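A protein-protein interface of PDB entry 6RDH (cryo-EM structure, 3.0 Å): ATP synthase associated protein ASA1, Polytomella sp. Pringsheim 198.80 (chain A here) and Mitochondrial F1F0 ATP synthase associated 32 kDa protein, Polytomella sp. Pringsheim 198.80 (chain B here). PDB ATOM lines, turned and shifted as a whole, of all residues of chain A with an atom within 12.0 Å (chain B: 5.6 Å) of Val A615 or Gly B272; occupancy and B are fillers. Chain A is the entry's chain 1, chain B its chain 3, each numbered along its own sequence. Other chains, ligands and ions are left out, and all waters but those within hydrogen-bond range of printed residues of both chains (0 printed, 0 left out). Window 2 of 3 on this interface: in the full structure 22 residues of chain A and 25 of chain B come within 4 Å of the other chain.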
ATOM      1  N   ARG A 600      34.859  23.261  18.283  1.00  0.00           N
ATOM      2  CA  ARG A 600      34.650  22.390  19.430  1.00  0.00           C
ATOM      3  C   ARG A 600      35.745  22.577  20.466  1.00  0.00           C
ATOM      4  O   ARG A 600      35.468  22.595  21.667  1.00  0.00           O
ATOM      5  CB  ARG A 600      34.588  20.935  18.976  1.00  0.00           C
ATOM      6  CG  ARG A 600      34.308  19.950  20.088  1.00  0.00           C
ATOM      7  CD  ARG A 600      34.259  18.528  19.586  1.00  0.00           C
ATOM      8  NE  ARG A 600      33.363  18.398  18.451  1.00  0.00           N
ATOM      9  CZ  ARG A 600      33.691  17.803  17.314  1.00  0.00           C
ATOM     10  NH1 ARG A 600      34.892  17.270  17.171  1.00  0.00           N
ATOM     11  NH2 ARG A 600      32.817  17.733  16.326  1.00  0.00           N
ATOM     12  N   ARG A 604      35.344  24.010  24.208  1.00  0.00           N
ATOM     13  CA  ARG A 604      35.873  23.246  25.326  1.00  0.00           C
ATOM     14  C   ARG A 604      36.888  24.041  26.129  1.00  0.00           C
ATOM     15  O   ARG A 604      37.074  23.766  27.319  1.00  0.00           O
ATOM     16  CB  ARG A 604      36.500  21.947  24.830  1.00  0.00           C
ATOM     17  CG  ARG A 604      36.428  20.800  25.813  1.00  0.00           C
ATOM     18  CD  ARG A 604      36.424  19.489  25.070  1.00  0.00           C
ATOM     19  NE  ARG A 604      35.373  19.470  24.063  1.00  0.00           N
ATOM     20  CZ  ARG A 604      34.160  18.968  24.256  1.00  0.00           C
ATOM     21  NH1 ARG A 604      33.845  18.419  25.416  1.00  0.00           N
ATOM     22  NH2 ARG A 604      33.264  19.005  23.285  1.00  0.00           N
ATOM     23  N   ARG A 609      29.690  23.735  25.627  1.00  0.00           N
ATOM     24  CA  ARG A 609      29.644  22.640  24.677  1.00  0.00           C
ATOM     25  C   ARG A 609      29.351  23.181  23.286  1.00  0.00           C
ATOM     26  O   ARG A 609      28.676  24.201  23.130  1.00  0.00           O
ATOM     27  CB  ARG A 609      28.587  21.615  25.080  1.00  0.00           C
ATOM     28  CG  ARG A 609      28.884  20.932  26.399  1.00  0.00           C
ATOM     29  CD  ARG A 609      27.613  20.535  27.105  1.00  0.00           C
ATOM     30  NE  ARG A 609      26.903  19.463  26.421  1.00  0.00           N
ATOM     31  CZ  ARG A 609      25.754  18.956  26.845  1.00  0.00           C
ATOM     32  NH1 ARG A 609      25.168  17.978  26.174  1.00  0.00           N
ATOM     33  NH2 ARG A 609      25.192  19.430  27.948  1.00  0.00           N
ATOM     34  N   TYR A 610      29.875  22.493  22.277  1.00  0.00           N
ATOM     35  CA  TYR A 610      29.647  22.904  20.900  1.00  0.00           C
ATOM     36  C   TYR A 610      28.208  22.601  20.504  1.00  0.00           C
ATOM     37  O   TYR A 610      27.715  21.489  20.712  1.00  0.00           O
ATOM     38  CB  TYR A 610      30.633  22.204  19.971  1.00  0.00           C
ATOM     39  CG  TYR A 610      30.622  22.725  18.556  1.00  0.00           C
ATOM     40  CD1 TYR A 610      30.379  24.061  18.288  1.00  0.00           C
ATOM     41  CD2 TYR A 610      30.861  21.879  17.488  1.00  0.00           C
ATOM     42  CE1 TYR A 610      30.366  24.535  16.998  1.00  0.00           C
ATOM     43  CE2 TYR A 610      30.845  22.343  16.198  1.00  0.00           C
ATOM     44  CZ  TYR A 610      30.599  23.670  15.959  1.00  0.00           C
ATOM     45  OH  TYR A 610      30.588  24.139  14.669  1.00  0.00           O
ATOM     46  N   GLY A 611      27.537  23.608  19.956  1.00  0.00           N
ATOM     47  CA  GLY A 611      26.129  23.569  19.628  1.00  0.00           C
ATOM     48  C   GLY A 611      25.649  22.470  18.696  1.00  0.00           C
ATOM     49  O   GLY A 611      24.724  21.729  19.035  1.00  0.00           O
ATOM     50  N   PRO A 612      26.225  22.361  17.492  1.00  0.00           N
ATOM     51  CA  PRO A 612      25.793  21.301  16.563  1.00  0.00           C
ATOM     52  C   PRO A 612      26.114  19.876  16.997  1.00  0.00           C
ATOM     53  O   PRO A 612      25.597  18.942  16.372  1.00  0.00           O
ATOM     54  CB  PRO A 612      26.535  21.653  15.275  1.00  0.00           C
ATOM     55  CG  PRO A 612      26.684  23.099  15.343  1.00  0.00           C
ATOM     56  CD  PRO A 612      26.956  23.414  16.769  1.00  0.00           C
ATOM     57  N   ASP A 613      26.925  19.666  18.032  1.00  0.00           N
ATOM     58  CA  ASP A 613      27.164  18.319  18.535  1.00  0.00           C
ATOM     59  C   ASP A 613      26.028  17.793  19.396  1.00  0.00           C
ATOM     60  O   ASP A 613      26.108  16.652  19.854  1.00  0.00           O
ATOM     61  CB  ASP A 613      28.454  18.271  19.349  1.00  0.00           C
ATOM     62  CG  ASP A 613      29.686  18.482  18.505  1.00  0.00           C
ATOM     63  OD1 ASP A 613      29.544  18.677  17.283  1.00  0.00           O
ATOM     64  OD2 ASP A 613      30.800  18.454  19.066  1.00  0.00           O
ATOM     65  N   LEU A 614      24.989  18.582  19.632  1.00  0.00           N
ATOM     66  CA  LEU A 614      23.910  18.223  20.538  1.00  0.00           C
ATOM     67  C   LEU A 614      22.679  17.786  19.760  1.00  0.00           C
ATOM     68  O   LEU A 614      22.503  18.129  18.591  1.00  0.00           O
ATOM     69  CB  LEU A 614      23.564  19.398  21.452  1.00  0.00           C
ATOM     70  CG  LEU A 614      24.763  20.071  22.120  1.00  0.00           C
ATOM     71  CD1 LEU A 614      24.313  21.254  22.944  1.00  0.00           C
ATOM     72  CD2 LEU A 614      25.526  19.080  22.972  1.00  0.00           C
ATOM     73  N   VAL A 615      21.820  17.024  20.432  1.00  0.00           N
ATOM     74  CA  VAL A 615      20.673  16.416  19.762  1.00  0.00           C
ATOM     75  C   VAL A 615      19.584  17.449  19.500  1.00  0.00           C
ATOM     76  O   VAL A 615      19.200  17.697  18.352  1.00  0.00           O
ATOM     77  CB  VAL A 615      20.136  15.231  20.582  1.00  0.00           C
ATOM     78  CG1 VAL A 615      18.833  14.743  19.995  1.00  0.00           C
ATOM     79  CG2 VAL A 615      21.155  14.113  20.605  1.00  0.00           C
ATOM     80  N   ASN A 616      19.066  18.061  20.557  1.00  0.00           N
ATOM     81  CA  ASN A 616      18.002  19.044  20.433  1.00  0.00           C
ATOM     82  C   ASN A 616      18.508  20.465  20.602  1.00  0.00           C
ATOM     83  O   ASN A 616      17.702  21.385  20.761  1.00  0.00           O
ATOM     84  CB  ASN A 616      16.891  18.745  21.445  1.00  0.00           C
ATOM     85  CG  ASN A 616      17.432  18.304  22.796  1.00  0.00           C
ATOM     86  OD1 ASN A 616      18.534  18.680  23.196  1.00  0.00           O
ATOM     87  ND2 ASN A 616      16.660  17.489  23.498  1.00  0.00           N
ATOM     88  N   GLY A 617      19.822  20.662  20.570  1.00  0.00           N
ATOM     89  CA  GLY A 617      20.410  21.976  20.736  1.00  0.00           C
ATOM     90  C   GLY A 617      21.615  22.209  19.847  1.00  0.00           C
ATOM     91  O   GLY A 617      21.757  21.573  18.804  1.00  0.00           O
ATOM     92  N   GLU B 232      27.399  12.984  24.089  1.00  0.00           N
ATOM     93  CA  GLU B 232      26.352  13.261  23.119  1.00  0.00           C
ATOM     94  C   GLU B 232      26.983  13.840  21.865  1.00  0.00           C
ATOM     95  O   GLU B 232      27.591  14.914  21.909  1.00  0.00           O
ATOM     96  CB  GLU B 232      25.320  14.218  23.701  1.00  0.00           C
ATOM     97  CG  GLU B 232      24.194  14.574  22.762  1.00  0.00           C
ATOM     98  CD  GLU B 232      23.141  15.428  23.438  1.00  0.00           C
ATOM     99  OE1 GLU B 232      22.950  15.281  24.663  1.00  0.00           O
ATOM    100  OE2 GLU B 232      22.505  16.250  22.753  1.00  0.00           O
ATOM    101  N   ALA B 234      25.446  14.182  18.135  1.00  0.00           N
ATOM    102  CA  ALA B 234      24.270  13.921  17.308  1.00  0.00           C
ATOM    103  C   ALA B 234      24.632  13.608  15.865  1.00  0.00           C
ATOM    104  O   ALA B 234      23.868  12.928  15.170  1.00  0.00           O
ATOM    105  CB  ALA B 234      23.322  15.110  17.343  1.00  0.00           C
ATOM    106  N   LEU B 237      25.440  10.002  16.034  1.00  0.00           N
ATOM    107  CA  LEU B 237      24.224   9.228  16.243  1.00  0.00           C
ATOM    108  C   LEU B 237      23.412   9.127  14.964  1.00  0.00           C
ATOM    109  O   LEU B 237      22.885   8.059  14.648  1.00  0.00           O
ATOM    110  CB  LEU B 237      23.388   9.841  17.360  1.00  0.00           C
ATOM    111  CG  LEU B 237      23.983   9.919  18.761  1.00  0.00           C
ATOM    112  CD1 LEU B 237      22.969  10.528  19.687  1.00  0.00           C
ATOM    113  CD2 LEU B 237      24.443   8.579  19.267  1.00  0.00           C
ATOM    114  N   ALA B 267      20.418   3.077  24.389  1.00  0.00           N
ATOM    115  CA  ALA B 267      21.338   4.159  24.071  1.00  0.00           C
ATOM    116  C   ALA B 267      20.704   5.237  23.201  1.00  0.00           C
ATOM    117  O   ALA B 267      21.249   6.338  23.117  1.00  0.00           O
ATOM    118  CB  ALA B 267      22.580   3.600  23.394  1.00  0.00           C
ATOM    119  N   PHE B 268      19.579   4.954  22.548  1.00  0.00           N
ATOM    120  CA  PHE B 268      18.852   6.000  21.845  1.00  0.00           C
ATOM    121  C   PHE B 268      17.970   6.815  22.774  1.00  0.00           C
ATOM    122  O   PHE B 268      17.794   8.015  22.548  1.00  0.00           O
ATOM    123  CB  PHE B 268      18.014   5.400  20.717  1.00  0.00           C
ATOM    124  CG  PHE B 268      18.763   5.211  19.430  1.00  0.00           C
ATOM    125  CD1 PHE B 268      19.863   5.997  19.132  1.00  0.00           C
ATOM    126  CD2 PHE B 268      18.378   4.240  18.528  1.00  0.00           C
ATOM    127  CE1 PHE B 268      20.548   5.831  17.950  1.00  0.00           C
ATOM    128  CE2 PHE B 268      19.064   4.062  17.350  1.00  0.00           C
ATOM    129  CZ  PHE B 268      20.146   4.860  17.060  1.00  0.00           C
ATOM    130  N   GLN B 269      17.399   6.200  23.811  1.00  0.00           N
ATOM    131  CA  GLN B 269      16.620   6.988  24.758  1.00  0.00           C
ATOM    132  C   GLN B 269      17.504   7.708  25.763  1.00  0.00           C
ATOM    133  O   GLN B 269      17.055   8.688  26.366  1.00  0.00           O
ATOM    134  CB  GLN B 269      15.588   6.105  25.476  1.00  0.00           C
ATOM    135  CG  GLN B 269      16.148   5.032  26.403  1.00  0.00           C
ATOM    136  CD  GLN B 269      16.210   5.458  27.857  1.00  0.00           C
ATOM    137  OE1 GLN B 269      15.365   6.221  28.326  1.00  0.00           O
ATOM    138  NE2 GLN B 269      17.211   4.967  28.577  1.00  0.00           N
ATOM    139  N   THR B 270      18.745   7.247  25.941  1.00  0.00           N
ATOM    140  CA  THR B 270      19.690   7.945  26.807  1.00  0.00           C
ATOM    141  C   THR B 270      20.052   9.313  26.246  1.00  0.00           C
ATOM    142  O   THR B 270      20.120  10.299  26.987  1.00  0.00           O
ATOM    143  CB  THR B 270      20.938   7.085  26.991  1.00  0.00           C
ATOM    144  OG1 THR B 270      20.558   5.810  27.511  1.00  0.00           O
ATOM    145  CG2 THR B 270      21.915   7.729  27.944  1.00  0.00           C
ATOM    146  N   PHE B 271      20.266   9.402  24.939  1.00  0.00           N
ATOM    147  CA  PHE B 271      20.610  10.665  24.306  1.00  0.00           C
ATOM    148  C   PHE B 271      19.399  11.477  23.889  1.00  0.00           C
ATOM    149  O   PHE B 271      19.553  12.646  23.529  1.00  0.00           O
ATOM    150  CB  PHE B 271      21.485  10.425  23.080  1.00  0.00           C
ATOM    151  CG  PHE B 271      22.849   9.928  23.410  1.00  0.00           C
ATOM    152  CD1 PHE B 271      23.685  10.668  24.218  1.00  0.00           C
ATOM    153  CD2 PHE B 271      23.298   8.725  22.907  1.00  0.00           C
ATOM    154  CE1 PHE B 271      24.944  10.213  24.526  1.00  0.00           C
ATOM    155  CE2 PHE B 271      24.557   8.267  23.212  1.00  0.00           C
ATOM    156  CZ  PHE B 271      25.379   9.015  24.017  1.00  0.00           C
ATOM    157  N   GLY B 272      18.208  10.891  23.926  1.00  0.00           N
ATOM    158  CA  GLY B 272      17.034  11.592  23.459  1.00  0.00           C
ATOM    159  C   GLY B 272      17.000  11.800  21.971  1.00  0.00           C
ATOM    160  O   GLY B 272      16.316  12.710  21.497  1.00  0.00           O
ATOM    161  N   PHE B 273      17.730  10.986  21.216  1.00  0.00           N
ATOM    162  CA  PHE B 273      17.819  11.119  19.772  1.00  0.00           C
ATOM    163  C   PHE B 273      16.975  10.033  19.130  1.00  0.00           C
ATOM    164  O   PHE B 273      17.268   8.844  19.279  1.00  0.00           O
ATOM    165  CB  PHE B 273      19.269  11.026  19.302  1.00  0.00           C
ATOM    166  CG  PHE B 273      19.425  11.158  17.822  1.00  0.00           C
ATOM    167  CD1 PHE B 273      19.854  10.088  17.061  1.00  0.00           C
ATOM    168  CD2 PHE B 273      19.107  12.345  17.187  1.00  0.00           C
ATOM    169  CE1 PHE B 273      19.979  10.207  15.701  1.00  0.00           C
ATOM    170  CE2 PHE B 273      19.230  12.465  15.830  1.00  0.00           C
ATOM    171  CZ  PHE B 273      19.667  11.394  15.086  1.00  0.00           C
ATOM    172  N   TYR B 274      15.931  10.443  18.414  1.00  0.00           N
ATOM    173  CA  TYR B 274      14.983   9.522  17.797  1.00  0.00           C
ATOM    174  C   TYR B 274      14.982   9.750  16.293  1.00  0.00           C
ATOM    175  O   TYR B 274      14.142  10.494  15.766  1.00  0.00           O
ATOM    176  CB  TYR B 274      13.594   9.699  18.401  1.00  0.00           C
ATOM    177  CG  TYR B 274      13.612   9.500  19.893  1.00  0.00           C
ATOM    178  CD1 TYR B 274      13.842   8.242  20.432  1.00  0.00           C
ATOM    179  CD2 TYR B 274      13.429  10.565  20.763  1.00  0.00           C
ATOM    180  CE1 TYR B 274      13.882   8.046  21.792  1.00  0.00           C
ATOM    181  CE2 TYR B 274      13.464  10.376  22.132  1.00  0.00           C
ATOM    182  CZ  TYR B 274      13.691   9.113  22.636  1.00  0.00           C
ATOM    183  OH  TYR B 274      13.727   8.905  23.992  1.00  0.00           O
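NH1 of Arg A609 lies within salt-bridge range of OE1 of Glu B232 (3.8 Å).
N of Ala B234 is in hydrogen-bond range of O of Asp A613.
The backbone carbonyl oxygen of Asp A613 lies close to the backbone carbonyl oxygen of Glu B232.
The side-chain carboxylate (OE2) of Glu B232 sits at hydrogen-bond distance from the backbone NH (N) of Val A615.
Along chain B the printed residues that touch a printed residue of chain A span positions 232 to 273.
Of the 11 printed residues of chain A, 4 touch a printed residue of chain B.
Among the printed residues, 10 pairs touch across the chains.
The guanidinium group (NE) of Arg A600 lies within salt-bridge range of the side-chain carboxylate (OD2) of Asp A613.
The backbone carbonyl oxygen (O) of Phe B268 lies within hydrogen-bond range of the backbone NH (N) of Phe B273 (3.3 Å).
OE2 of Glu B232 touches CA of Leu A614 (3.3 Å).
Ala B234 touches Leu A614 (CB to O, 3.4 Å).
Val A615 touches Ala B234.
Phe B271 touches Val A615 (O to CG2, 3.6 Å).
Val A615 touches Gly B272 (CG1 to O, 3.6 Å).
Val A615 touches Phe B273 (CG1 to CD2, 3.7 Å).
Of chain B, only Glu B232 (2.5 Å), Ala B234 (3.8 Å), Phe B271 (3.6 Å), Gly B272 (3.6 Å) and Phe B273 (3.7 Å) come within 4 Å of Val A615.
Of the printed residues of chain A, Gly B272 touches Val A615 (3.6 Å).
Glu B232 touches just these residues of chain A: Arg A609, Asp A613, Leu A614 and Val A615.
Of chain A, only Asp A613, Leu A614 and Val A615 come within 4 Å of Ala B234.
No residue of chain A comes within 4 Å of Gln B269.
Thr B270 touches none of the printed residues of chain A.
Of chain A, only Val A615 (3.6 Å) comes within 4 Å of Phe B271.
Printed residues of chain A within 4 Å of Phe B273: Val A615 (3.7 Å).
No residue of chain A comes within 4 Å of Tyr B274.
Printed residues of chain B within 4 Å of Arg A609: Glu B232.
Of the printed residues of chain B, Leu A614 touches Glu B232 (3.3 Å) and Ala B234 (3.4 Å).
Of the printed residues of chain B, Asp A613 touches Glu B232 and Ala B234.
Phe B268 touches none of the printed residues of chain A.
The nearest residue of chain A that does not touch Gly B272 is Asn A616 (5.2 Å).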
